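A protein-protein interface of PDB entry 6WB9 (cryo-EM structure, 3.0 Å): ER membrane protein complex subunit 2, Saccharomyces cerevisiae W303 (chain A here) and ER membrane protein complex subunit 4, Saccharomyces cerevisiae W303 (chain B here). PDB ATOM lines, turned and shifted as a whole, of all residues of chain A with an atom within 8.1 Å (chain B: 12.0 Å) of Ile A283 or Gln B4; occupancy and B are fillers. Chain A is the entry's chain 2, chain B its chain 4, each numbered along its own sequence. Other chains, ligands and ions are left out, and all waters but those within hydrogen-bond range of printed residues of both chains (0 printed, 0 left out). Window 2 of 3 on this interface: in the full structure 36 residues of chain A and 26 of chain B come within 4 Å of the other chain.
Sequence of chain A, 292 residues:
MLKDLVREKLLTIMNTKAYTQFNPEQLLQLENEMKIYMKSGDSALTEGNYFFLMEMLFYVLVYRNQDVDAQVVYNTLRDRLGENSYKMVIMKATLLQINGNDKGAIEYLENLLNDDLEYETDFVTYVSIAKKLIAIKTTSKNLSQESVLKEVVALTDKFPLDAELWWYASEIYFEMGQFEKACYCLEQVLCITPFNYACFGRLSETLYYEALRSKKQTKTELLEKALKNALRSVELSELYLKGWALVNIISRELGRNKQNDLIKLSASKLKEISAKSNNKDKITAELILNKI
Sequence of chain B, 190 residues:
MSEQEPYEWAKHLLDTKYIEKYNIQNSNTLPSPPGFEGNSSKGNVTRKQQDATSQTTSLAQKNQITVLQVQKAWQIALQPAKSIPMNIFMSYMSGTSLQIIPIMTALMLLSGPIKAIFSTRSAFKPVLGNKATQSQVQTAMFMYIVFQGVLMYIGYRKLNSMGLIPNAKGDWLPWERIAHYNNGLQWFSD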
ATOM      1  N   ASN A  23     -39.399  16.874 -22.262  1.00  0.00           N
ATOM      2  CA  ASN A  23     -40.400  17.865 -21.910  1.00  0.00           C
ATOM      3  C   ASN A  23     -41.586  17.765 -22.867  1.00  0.00           C
ATOM      4  O   ASN A  23     -41.471  17.172 -23.940  1.00  0.00           O
ATOM      5  CB  ASN A  23     -39.790  19.266 -21.968  1.00  0.00           C
ATOM      6  CG  ASN A  23     -38.613  19.427 -21.035  1.00  0.00           C
ATOM      7  OD1 ASN A  23     -37.560  19.929 -21.427  1.00  0.00           O
ATOM      8  ND2 ASN A  23     -38.781  18.998 -19.790  1.00  0.00           N
ATOM      9  N   GLN A  26     -40.444  19.432 -25.881  1.00  0.00           N
ATOM     10  CA  GLN A  26     -39.548  18.524 -26.584  1.00  0.00           C
ATOM     11  C   GLN A  26     -40.301  17.342 -27.174  1.00  0.00           C
ATOM     12  O   GLN A  26     -39.945  16.871 -28.256  1.00  0.00           O
ATOM     13  CB  GLN A  26     -38.445  18.045 -25.644  1.00  0.00           C
ATOM     14  CG  GLN A  26     -37.516  19.152 -25.181  1.00  0.00           C
ATOM     15  CD  GLN A  26     -36.480  18.671 -24.189  1.00  0.00           C
ATOM     16  OE1 GLN A  26     -36.436  17.493 -23.842  1.00  0.00           O
ATOM     17  NE2 GLN A  26     -35.643  19.586 -23.721  1.00  0.00           N
ATOM     18  N   LEU A 241     -19.658  15.041 -18.426  1.00  0.00           N
ATOM     19  CA  LEU A 241     -19.822  16.241 -17.613  1.00  0.00           C
ATOM     20  C   LEU A 241     -20.085  15.898 -16.153  1.00  0.00           C
ATOM     21  O   LEU A 241     -19.537  16.546 -15.254  1.00  0.00           O
ATOM     22  CB  LEU A 241     -20.958  17.088 -18.178  1.00  0.00           C
ATOM     23  CG  LEU A 241     -21.610  18.117 -17.263  1.00  0.00           C
ATOM     24  CD1 LEU A 241     -20.719  19.331 -17.086  1.00  0.00           C
ATOM     25  CD2 LEU A 241     -22.957  18.498 -17.826  1.00  0.00           C
ATOM     26  N   ILE A 273     -15.461  20.917 -21.788  1.00  0.00           N
ATOM     27  CA  ILE A 273     -16.869  20.565 -21.959  1.00  0.00           C
ATOM     28  C   ILE A 273     -17.714  21.818 -22.172  1.00  0.00           C
ATOM     29  O   ILE A 273     -18.593  21.849 -23.041  1.00  0.00           O
ATOM     30  CB  ILE A 273     -17.347  19.733 -20.752  1.00  0.00           C
ATOM     31  CG1 ILE A 273     -16.738  18.333 -20.810  1.00  0.00           C
ATOM     32  CG2 ILE A 273     -18.860  19.629 -20.698  1.00  0.00           C
ATOM     33  CD1 ILE A 273     -16.856  17.569 -19.521  1.00  0.00           C
ATOM     34  N   SER A 274     -17.433  22.889 -21.424  1.00  0.00           N
ATOM     35  CA  SER A 274     -18.105  24.163 -21.661  1.00  0.00           C
ATOM     36  C   SER A 274     -17.724  24.783 -23.000  1.00  0.00           C
ATOM     37  O   SER A 274     -18.485  25.597 -23.532  1.00  0.00           O
ATOM     38  CB  SER A 274     -17.789  25.140 -20.531  1.00  0.00           C
ATOM     39  OG  SER A 274     -18.328  26.420 -20.804  1.00  0.00           O
ATOM     40  N   SER A 277     -19.079  21.065 -25.907  1.00  0.00           N
ATOM     41  CA  SER A 277     -20.281  20.248 -25.793  1.00  0.00           C
ATOM     42  C   SER A 277     -21.540  21.095 -25.979  1.00  0.00           C
ATOM     43  O   SER A 277     -21.483  22.294 -26.264  1.00  0.00           O
ATOM     44  CB  SER A 277     -20.306  19.509 -24.458  1.00  0.00           C
ATOM     45  OG  SER A 277     -21.368  18.576 -24.412  1.00  0.00           O
ATOM     46  N   ASN A 278     -22.698  20.456 -25.813  1.00  0.00           N
ATOM     47  CA  ASN A 278     -23.981  21.089 -26.086  1.00  0.00           C
ATOM     48  C   ASN A 278     -24.309  22.143 -25.028  1.00  0.00           C
ATOM     49  O   ASN A 278     -23.609  22.300 -24.024  1.00  0.00           O
ATOM     50  CB  ASN A 278     -25.094  20.044 -26.158  1.00  0.00           C
ATOM     51  CG  ASN A 278     -25.086  19.096 -24.977  1.00  0.00           C
ATOM     52  OD1 ASN A 278     -24.039  18.602 -24.572  1.00  0.00           O
ATOM     53  ND2 ASN A 278     -26.261  18.837 -24.418  1.00  0.00           N
ATOM     54  N   ASN A 279     -25.404  22.872 -25.275  1.00  0.00           N
ATOM     55  CA  ASN A 279     -25.729  24.050 -24.474  1.00  0.00           C
ATOM     56  C   ASN A 279     -26.136  23.689 -23.052  1.00  0.00           C
ATOM     57  O   ASN A 279     -25.845  24.447 -22.121  1.00  0.00           O
ATOM     58  CB  ASN A 279     -26.836  24.857 -25.150  1.00  0.00           C
ATOM     59  CG  ASN A 279     -26.345  25.603 -26.374  1.00  0.00           C
ATOM     60  OD1 ASN A 279     -26.798  25.355 -27.491  1.00  0.00           O
ATOM     61  ND2 ASN A 279     -25.411  26.524 -26.169  1.00  0.00           N
ATOM     62  N   LYS A 280     -26.791  22.542 -22.863  1.00  0.00           N
ATOM     63  CA  LYS A 280     -27.106  22.089 -21.512  1.00  0.00           C
ATOM     64  C   LYS A 280     -25.839  21.721 -20.750  1.00  0.00           C
ATOM     65  O   LYS A 280     -25.672  22.114 -19.588  1.00  0.00           O
ATOM     66  CB  LYS A 280     -28.066  20.903 -21.570  1.00  0.00           C
ATOM     67  CG  LYS A 280     -28.484  20.392 -20.210  1.00  0.00           C
ATOM     68  CD  LYS A 280     -29.333  21.404 -19.473  1.00  0.00           C
ATOM     69  CE  LYS A 280     -30.775  21.337 -19.929  1.00  0.00           C
ATOM     70  NZ  LYS A 280     -31.381  20.015 -19.615  1.00  0.00           N
ATOM     71  N   ASP A 281     -24.919  21.004 -21.406  1.00  0.00           N
ATOM     72  CA  ASP A 281     -23.632  20.685 -20.795  1.00  0.00           C
ATOM     73  C   ASP A 281     -22.794  21.935 -20.567  1.00  0.00           C
ATOM     74  O   ASP A 281     -22.083  22.030 -19.564  1.00  0.00           O
ATOM     75  CB  ASP A 281     -22.859  19.693 -21.663  1.00  0.00           C
ATOM     76  CG  ASP A 281     -23.330  18.267 -21.486  1.00  0.00           C
ATOM     77  OD1 ASP A 281     -24.405  18.061 -20.890  1.00  0.00           O
ATOM     78  OD2 ASP A 281     -22.619  17.346 -21.941  1.00  0.00           O
ATOM     79  N   LYS A 282     -22.882  22.911 -21.475  1.00  0.00           N
ATOM     80  CA  LYS A 282     -22.109  24.142 -21.338  1.00  0.00           C
ATOM     81  C   LYS A 282     -22.599  24.976 -20.160  1.00  0.00           C
ATOM     82  O   LYS A 282     -21.794  25.462 -19.355  1.00  0.00           O
ATOM     83  CB  LYS A 282     -22.179  24.942 -22.639  1.00  0.00           C
ATOM     84  CG  LYS A 282     -21.581  26.332 -22.567  1.00  0.00           C
ATOM     85  CD  LYS A 282     -21.524  26.967 -23.945  1.00  0.00           C
ATOM     86  CE  LYS A 282     -21.088  28.418 -23.867  1.00  0.00           C
ATOM     87  NZ  LYS A 282     -22.075  29.248 -23.124  1.00  0.00           N
ATOM     88  N   ILE A 283     -23.921  25.125 -20.031  1.00  0.00           N
ATOM     89  CA  ILE A 283     -24.498  25.876 -18.921  1.00  0.00           C
ATOM     90  C   ILE A 283     -24.253  25.156 -17.598  1.00  0.00           C
ATOM     91  O   ILE A 283     -23.919  25.787 -16.585  1.00  0.00           O
ATOM     92  CB  ILE A 283     -25.995  26.129 -19.191  1.00  0.00           C
ATOM     93  CG1 ILE A 283     -26.156  27.155 -20.313  1.00  0.00           C
ATOM     94  CG2 ILE A 283     -26.721  26.617 -17.951  1.00  0.00           C
ATOM     95  CD1 ILE A 283     -27.576  27.318 -20.797  1.00  0.00           C
ATOM     96  N   THR A 284     -24.332  23.821 -17.598  1.00  0.00           N
ATOM     97  CA  THR A 284     -24.074  23.062 -16.378  1.00  0.00           C
ATOM     98  C   THR A 284     -22.600  23.118 -15.980  1.00  0.00           C
ATOM     99  O   THR A 284     -22.280  23.205 -14.790  1.00  0.00           O
ATOM    100  CB  THR A 284     -24.536  21.621 -16.572  1.00  0.00           C
ATOM    101  OG1 THR A 284     -25.868  21.616 -17.097  1.00  0.00           O
ATOM    102  CG2 THR A 284     -24.526  20.865 -15.263  1.00  0.00           C
ATOM    103  N   ALA A 285     -21.688  23.115 -16.955  1.00  0.00           N
ATOM    104  CA  ALA A 285     -20.267  23.205 -16.638  1.00  0.00           C
ATOM    105  C   ALA A 285     -19.885  24.598 -16.157  1.00  0.00           C
ATOM    106  O   ALA A 285     -19.026  24.732 -15.279  1.00  0.00           O
ATOM    107  CB  ALA A 285     -19.429  22.815 -17.854  1.00  0.00           C
ATOM    108  N   GLU A 286     -20.515  25.641 -16.707  1.00  0.00           N
ATOM    109  CA  GLU A 286     -20.308  26.980 -16.167  1.00  0.00           C
ATOM    110  C   GLU A 286     -20.947  27.136 -14.791  1.00  0.00           C
ATOM    111  O   GLU A 286     -20.514  27.981 -14.003  1.00  0.00           O
ATOM    112  CB  GLU A 286     -20.852  28.035 -17.129  1.00  0.00           C
ATOM    113  CG  GLU A 286     -20.096  28.133 -18.445  1.00  0.00           C
ATOM    114  CD  GLU A 286     -18.665  28.605 -18.275  1.00  0.00           C
ATOM    115  OE1 GLU A 286     -18.400  29.419 -17.365  1.00  0.00           O
ATOM    116  OE2 GLU A 286     -17.799  28.160 -19.057  1.00  0.00           O
ATOM    117  N   LEU A 287     -21.977  26.342 -14.490  1.00  0.00           N
ATOM    118  CA  LEU A 287     -22.524  26.327 -13.137  1.00  0.00           C
ATOM    119  C   LEU A 287     -21.571  25.642 -12.162  1.00  0.00           C
ATOM    120  O   LEU A 287     -21.424  26.082 -11.017  1.00  0.00           O
ATOM    121  CB  LEU A 287     -23.885  25.634 -13.133  1.00  0.00           C
ATOM    122  CG  LEU A 287     -24.640  25.593 -11.803  1.00  0.00           C
ATOM    123  CD1 LEU A 287     -25.305  26.930 -11.516  1.00  0.00           C
ATOM    124  CD2 LEU A 287     -25.652  24.463 -11.783  1.00  0.00           C
ATOM    125  N   ILE A 288     -20.924  24.560 -12.601  1.00  0.00           N
ATOM    126  CA  ILE A 288     -20.000  23.827 -11.736  1.00  0.00           C
ATOM    127  C   ILE A 288     -18.736  24.644 -11.481  1.00  0.00           C
ATOM    128  O   ILE A 288     -18.271  24.753 -10.340  1.00  0.00           O
ATOM    129  CB  ILE A 288     -19.671  22.449 -12.346  1.00  0.00           C
ATOM    130  CG1 ILE A 288     -20.905  21.544 -12.370  1.00  0.00           C
ATOM    131  CG2 ILE A 288     -18.543  21.760 -11.588  1.00  0.00           C
ATOM    132  CD1 ILE A 288     -21.342  21.042 -11.022  1.00  0.00           C
ATOM    133  N   LEU A 289     -18.178  25.255 -12.532  1.00  0.00           N
ATOM    134  CA  LEU A 289     -16.887  25.929 -12.408  1.00  0.00           C
ATOM    135  C   LEU A 289     -16.993  27.237 -11.633  1.00  0.00           C
ATOM    136  O   LEU A 289     -16.119  27.551 -10.818  1.00  0.00           O
ATOM    137  CB  LEU A 289     -16.297  26.187 -13.793  1.00  0.00           C
ATOM    138  CG  LEU A 289     -15.732  24.979 -14.536  1.00  0.00           C
ATOM    139  CD1 LEU A 289     -15.363  25.367 -15.952  1.00  0.00           C
ATOM    140  CD2 LEU A 289     -14.526  24.425 -13.800  1.00  0.00           C
ATOM    141  N   ASN A 290     -18.051  28.014 -11.866  1.00  0.00           N
ATOM    142  CA  ASN A 290     -18.166  29.358 -11.313  1.00  0.00           C
ATOM    143  C   ASN A 290     -18.851  29.389  -9.952  1.00  0.00           C
ATOM    144  O   ASN A 290     -19.436  30.417  -9.586  1.00  0.00           O
ATOM    145  CB  ASN A 290     -18.900  30.271 -12.295  1.00  0.00           C
ATOM    146  CG  ASN A 290     -18.260  30.284 -13.669  1.00  0.00           C
ATOM    147  OD1 ASN A 290     -17.071  30.003 -13.815  1.00  0.00           O
ATOM    148  ND2 ASN A 290     -19.048  30.613 -14.685  1.00  0.00           N
ATOM    149  N   GLN B   4     -31.036  28.151 -21.680  1.00  0.00           N
ATOM    150  CA  GLN B   4     -31.677  27.103 -20.895  1.00  0.00           C
ATOM    151  C   GLN B   4     -31.239  27.167 -19.437  1.00  0.00           C
ATOM    152  O   GLN B   4     -30.385  27.972 -19.067  1.00  0.00           O
ATOM    153  CB  GLN B   4     -31.352  25.721 -21.469  1.00  0.00           C
ATOM    154  CG  GLN B   4     -31.708  25.542 -22.934  1.00  0.00           C
ATOM    155  CD  GLN B   4     -31.388  24.149 -23.439  1.00  0.00           C
ATOM    156  OE1 GLN B   4     -31.034  23.263 -22.663  1.00  0.00           O
ATOM    157  NE2 GLN B   4     -31.508  23.949 -24.746  1.00  0.00           N
ATOM    158  N   GLU B   5     -31.832  26.315 -18.620  1.00  0.00           N
ATOM    159  CA  GLU B   5     -31.455  26.123 -17.232  1.00  0.00           C
ATOM    160  C   GLU B   5     -30.596  24.870 -17.096  1.00  0.00           C
ATOM    161  O   GLU B   5     -30.780  23.908 -17.845  1.00  0.00           O
ATOM    162  CB  GLU B   5     -32.700  26.003 -16.348  1.00  0.00           C
ATOM    163  CG  GLU B   5     -33.525  27.279 -16.287  1.00  0.00           C
ATOM    164  CD  GLU B   5     -34.603  27.230 -15.225  1.00  0.00           C
ATOM    165  OE1 GLU B   5     -34.624  26.257 -14.443  1.00  0.00           O
ATOM    166  OE2 GLU B   5     -35.428  28.167 -15.171  1.00  0.00           O
ATOM    167  N   PRO B   6     -29.630  24.845 -16.156  1.00  0.00           N
ATOM    168  CA  PRO B   6     -28.713  23.698 -16.072  1.00  0.00           C
ATOM    169  C   PRO B   6     -29.348  22.412 -15.561  1.00  0.00           C
ATOM    170  O   PRO B   6     -30.556  22.352 -15.312  1.00  0.00           O
ATOM    171  CB  PRO B   6     -27.624  24.194 -15.111  1.00  0.00           C
ATOM    172  CG  PRO B   6     -28.274  25.258 -14.319  1.00  0.00           C
ATOM    173  CD  PRO B   6     -29.231  25.931 -15.244  1.00  0.00           C
ATOM    174  N   TYR B   7     -28.525  21.376 -15.417  1.00  0.00           N
ATOM    175  CA  TYR B   7     -29.006  20.057 -15.035  1.00  0.00           C
ATOM    176  C   TYR B   7     -29.499  20.037 -13.595  1.00  0.00           C
ATOM    177  O   TYR B   7     -29.088  20.846 -12.760  1.00  0.00           O
ATOM    178  CB  TYR B   7     -27.900  19.020 -15.194  1.00  0.00           C
ATOM    179  CG  TYR B   7     -27.807  18.384 -16.559  1.00  0.00           C
ATOM    180  CD1 TYR B   7     -28.882  17.692 -17.099  1.00  0.00           C
ATOM    181  CD2 TYR B   7     -26.631  18.447 -17.293  1.00  0.00           C
ATOM    182  CE1 TYR B   7     -28.795  17.099 -18.344  1.00  0.00           C
ATOM    183  CE2 TYR B   7     -26.533  17.856 -18.534  1.00  0.00           C
ATOM    184  CZ  TYR B   7     -27.617  17.184 -19.055  1.00  0.00           C
ATOM    185  OH  TYR B   7     -27.521  16.596 -20.295  1.00  0.00           O
ATOM    186  N   GLU B   8     -30.385  19.084 -13.308  1.00  0.00           N
ATOM    187  CA  GLU B   8     -30.956  18.974 -11.975  1.00  0.00           C
ATOM    188  C   GLU B   8     -30.044  18.235 -11.004  1.00  0.00           C
ATOM    189  O   GLU B   8     -30.183  18.417  -9.790  1.00  0.00           O
ATOM    190  CB  GLU B   8     -32.319  18.281 -12.047  1.00  0.00           C
ATOM    191  CG  GLU B   8     -33.266  18.662 -10.921  1.00  0.00           C
ATOM    192  CD  GLU B   8     -33.536  20.152 -10.869  1.00  0.00           C
ATOM    193  OE1 GLU B   8     -33.789  20.751 -11.936  1.00  0.00           O
ATOM    194  OE2 GLU B   8     -33.490  20.729  -9.762  1.00  0.00           O
ATOM    195  N   TRP B   9     -29.114  17.414 -11.501  1.00  0.00           N
ATOM    196  CA  TRP B   9     -28.156  16.785 -10.600  1.00  0.00           C
ATOM    197  C   TRP B   9     -27.122  17.772 -10.086  1.00  0.00           C
ATOM    198  O   TRP B   9     -26.538  17.535  -9.026  1.00  0.00           O
ATOM    199  CB  TRP B   9     -27.455  15.599 -11.277  1.00  0.00           C
ATOM    200  CG  TRP B   9     -26.746  15.920 -12.566  1.00  0.00           C
ATOM    201  CD1 TRP B   9     -27.230  15.742 -13.826  1.00  0.00           C
ATOM    202  CD2 TRP B   9     -25.422  16.454 -12.718  1.00  0.00           C
ATOM    203  NE1 TRP B   9     -26.297  16.135 -14.752  1.00  0.00           N
ATOM    204  CE2 TRP B   9     -25.180  16.581 -14.097  1.00  0.00           C
ATOM    205  CE3 TRP B   9     -24.417  16.836 -11.822  1.00  0.00           C
ATOM    206  CZ2 TRP B   9     -23.984  17.080 -14.600  1.00  0.00           C
ATOM    207  CZ3 TRP B   9     -23.236  17.336 -12.323  1.00  0.00           C
ATOM    208  CH2 TRP B   9     -23.029  17.457 -13.698  1.00  0.00           C
ATOM    209  N   ALA B  10     -26.881  18.870 -10.808  1.00  0.00           N
ATOM    210  CA  ALA B  10     -25.884  19.856 -10.414  1.00  0.00           C
ATOM    211  C   ALA B  10     -26.460  21.019  -9.626  1.00  0.00           C
ATOM    212  O   ALA B  10     -25.708  21.691  -8.912  1.00  0.00           O
ATOM    213  CB  ALA B  10     -25.158  20.405 -11.644  1.00  0.00           C
ATOM    214  N   LYS B  11     -27.763  21.283  -9.742  1.00  0.00           N
ATOM    215  CA  LYS B  11     -28.399  22.223  -8.827  1.00  0.00           C
ATOM    216  C   LYS B  11     -28.477  21.649  -7.422  1.00  0.00           C
ATOM    217  O   LYS B  11     -28.520  22.403  -6.444  1.00  0.00           O
ATOM    218  CB  LYS B  11     -29.798  22.590  -9.323  1.00  0.00           C
ATOM    219  CG  LYS B  11     -29.828  23.375 -10.621  1.00  0.00           C
ATOM    220  CD  LYS B  11     -31.262  23.620 -11.065  1.00  0.00           C
ATOM    221  CE  LYS B  11     -31.313  24.399 -12.367  1.00  0.00           C
ATOM    222  NZ  LYS B  11     -32.709  24.666 -12.808  1.00  0.00           N
ATOM    223  N   HIS B  12     -28.499  20.325  -7.307  1.00  0.00           N
ATOM    224  CA  HIS B  12     -28.532  19.630  -6.032  1.00  0.00           C
ATOM    225  C   HIS B  12     -27.152  19.195  -5.559  1.00  0.00           C
ATOM    226  O   HIS B  12     -27.041  18.601  -4.481  1.00  0.00           O
ATOM    227  CB  HIS B  12     -29.449  18.408  -6.132  1.00  0.00           C
ATOM    228  CG  HIS B  12     -30.858  18.734  -6.514  1.00  0.00           C
ATOM    229  ND1 HIS B  12     -31.413  19.981  -6.325  1.00  0.00           N
ATOM    230  CD2 HIS B  12     -31.827  17.974  -7.077  1.00  0.00           C
ATOM    231  CE1 HIS B  12     -32.663  19.975  -6.754  1.00  0.00           C
ATOM    232  NE2 HIS B  12     -32.938  18.768  -7.215  1.00  0.00           N
ATOM    233  N   LEU B  13     -26.100  19.467  -6.331  1.00  0.00           N
ATOM    234  CA  LEU B  13     -24.750  19.046  -5.975  1.00  0.00           C
ATOM    235  C   LEU B  13     -23.910  20.161  -5.376  1.00  0.00           C
ATOM    236  O   LEU B  13     -23.029  19.884  -4.556  1.00  0.00           O
ATOM    237  CB  LEU B  13     -24.020  18.496  -7.205  1.00  0.00           C
ATOM    238  CG  LEU B  13     -22.882  17.505  -6.968  1.00  0.00           C
ATOM    239  CD1 LEU B  13     -23.437  16.126  -6.671  1.00  0.00           C
ATOM    240  CD2 LEU B  13     -21.948  17.465  -8.162  1.00  0.00           C
ATOM    241  N   LEU B  14     -24.157  21.412  -5.764  1.00  0.00           N
ATOM    242  CA  LEU B  14     -23.340  22.515  -5.274  1.00  0.00           C
ATOM    243  C   LEU B  14     -23.735  22.923  -3.861  1.00  0.00           C
ATOM    244  O   LEU B  14     -22.867  23.208  -3.029  1.00  0.00           O
ATOM    245  CB  LEU B  14     -23.451  23.711  -6.218  1.00  0.00           C
ATOM    246  CG  LEU B  14     -23.091  23.451  -7.678  1.00  0.00           C
ATOM    247  CD1 LEU B  14     -23.128  24.747  -8.460  1.00  0.00           C
ATOM    248  CD2 LEU B  14     -21.729  22.798  -7.780  1.00  0.00           C
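Of the 11 printed residues of chain B, 7 touch a printed residue of chain A.
Printed residues of chain B that touch a printed residue of chain A: Gln B4, Glu B5, Pro B6, Tyr B7, Trp B9, Ala B10 and Leu B14.
Hydrophobic or aromatic side chains of chain B that line the printed part of chain A: Pro B6, Tyr B7, Trp B9, Ala B10 and Leu B14.
Hydrophobic or aromatic side chains of chain A within 4 Å of the printed part of chain B: Leu A241, Ile A283, Leu A287 and Ile A288.
Among the printed residues, no Asp or Glu carboxylate lies within 4 Å of a Lys or Arg side-chain nitrogen of the other chain.
Among the printed residues, pairs that only touch across the chains: Leu A241 with Tyr B7, Leu A241 with Trp B9, Lys A280 with Gln B4, Lys A280 with Glu B5, Lys A280 with Tyr B7, Ile A283 with Gln B4, Ile A283 with Pro B6, Thr A284 with Pro B6, Thr A284 with Trp B9, Thr A284 with Ala B10, Leu A287 with Pro B6, Leu A287 with Ala B10, Leu A287 with Leu B14, Ile A288 with Ala B10 and Ile A288 with Leu B14.
Of the printed residues of chain B, Leu A241 touches Tyr B7 and Trp B9.
Ile A273 touches none of the printed residues of chain B.
No residue of chain B comes within 4 Å of Ser A274.
Lys A280 touches just these residues of chain B: Gln B4, Glu B5 and Tyr B7.
No residue of chain B comes within 4 Å of Lys A282.
Of chain B, only Gln B4 and Pro B6 come within 4 Å of Ile A283.
Of chain B, only Pro B6 (3.7 Å), Tyr B7 (3.2 Å), Trp B9 (3.9 Å) and Ala B10 (3.7 Å) come within 4 Å of Thr A284.
No residue of chain B comes within 4 Å of Ala A285.
No residue of chain B comes within 4 Å of Glu A286.
Of the printed residues of chain B, Leu A287 touches Pro B6, Ala B10 and Leu B14.
Of chain A, only Lys A280 and Ile A283 come within 4 Å of Gln B4.
Of the printed residues of chain A, Pro B6 touches Ile A283, Thr A284 and Leu A287.
The nearest residue of chain B that does not touch Ile A283 is Glu B5 (4.3 Å).
The nearest residue of chain A that does not touch Gln B4 is Asn A279 (4.8 Å).
The nearest printed residue of chain B that does not touch Asp A281 is Trp B9 (6.4 Å).
OD1 of Asp A281 sits close to OH of Tyr B7, at 3.5 Å.
The backbone NH of Tyr B7 lies within hydrogen-bond range of the side-chain hydroxyl of Thr A284.
OD2 of Asp A281 sits at hydrogen-bond distance from OG of Ser A277, at 3.0 Å.
The side-chain amide oxygen of Asn A278 lies close to the side-chain carboxylate of Asp A281.
The side-chain hydroxyl (OG1) of Thr A284 sits at hydrogen-bond distance from the backbone carbonyl oxygen (O) of Lys A280 (2.5 Å).
The side-chain carboxylate (OE1) of Glu B5 is in salt-bridge range of the side-chain amino group (NZ) of Lys B11, at 3.0 Å.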
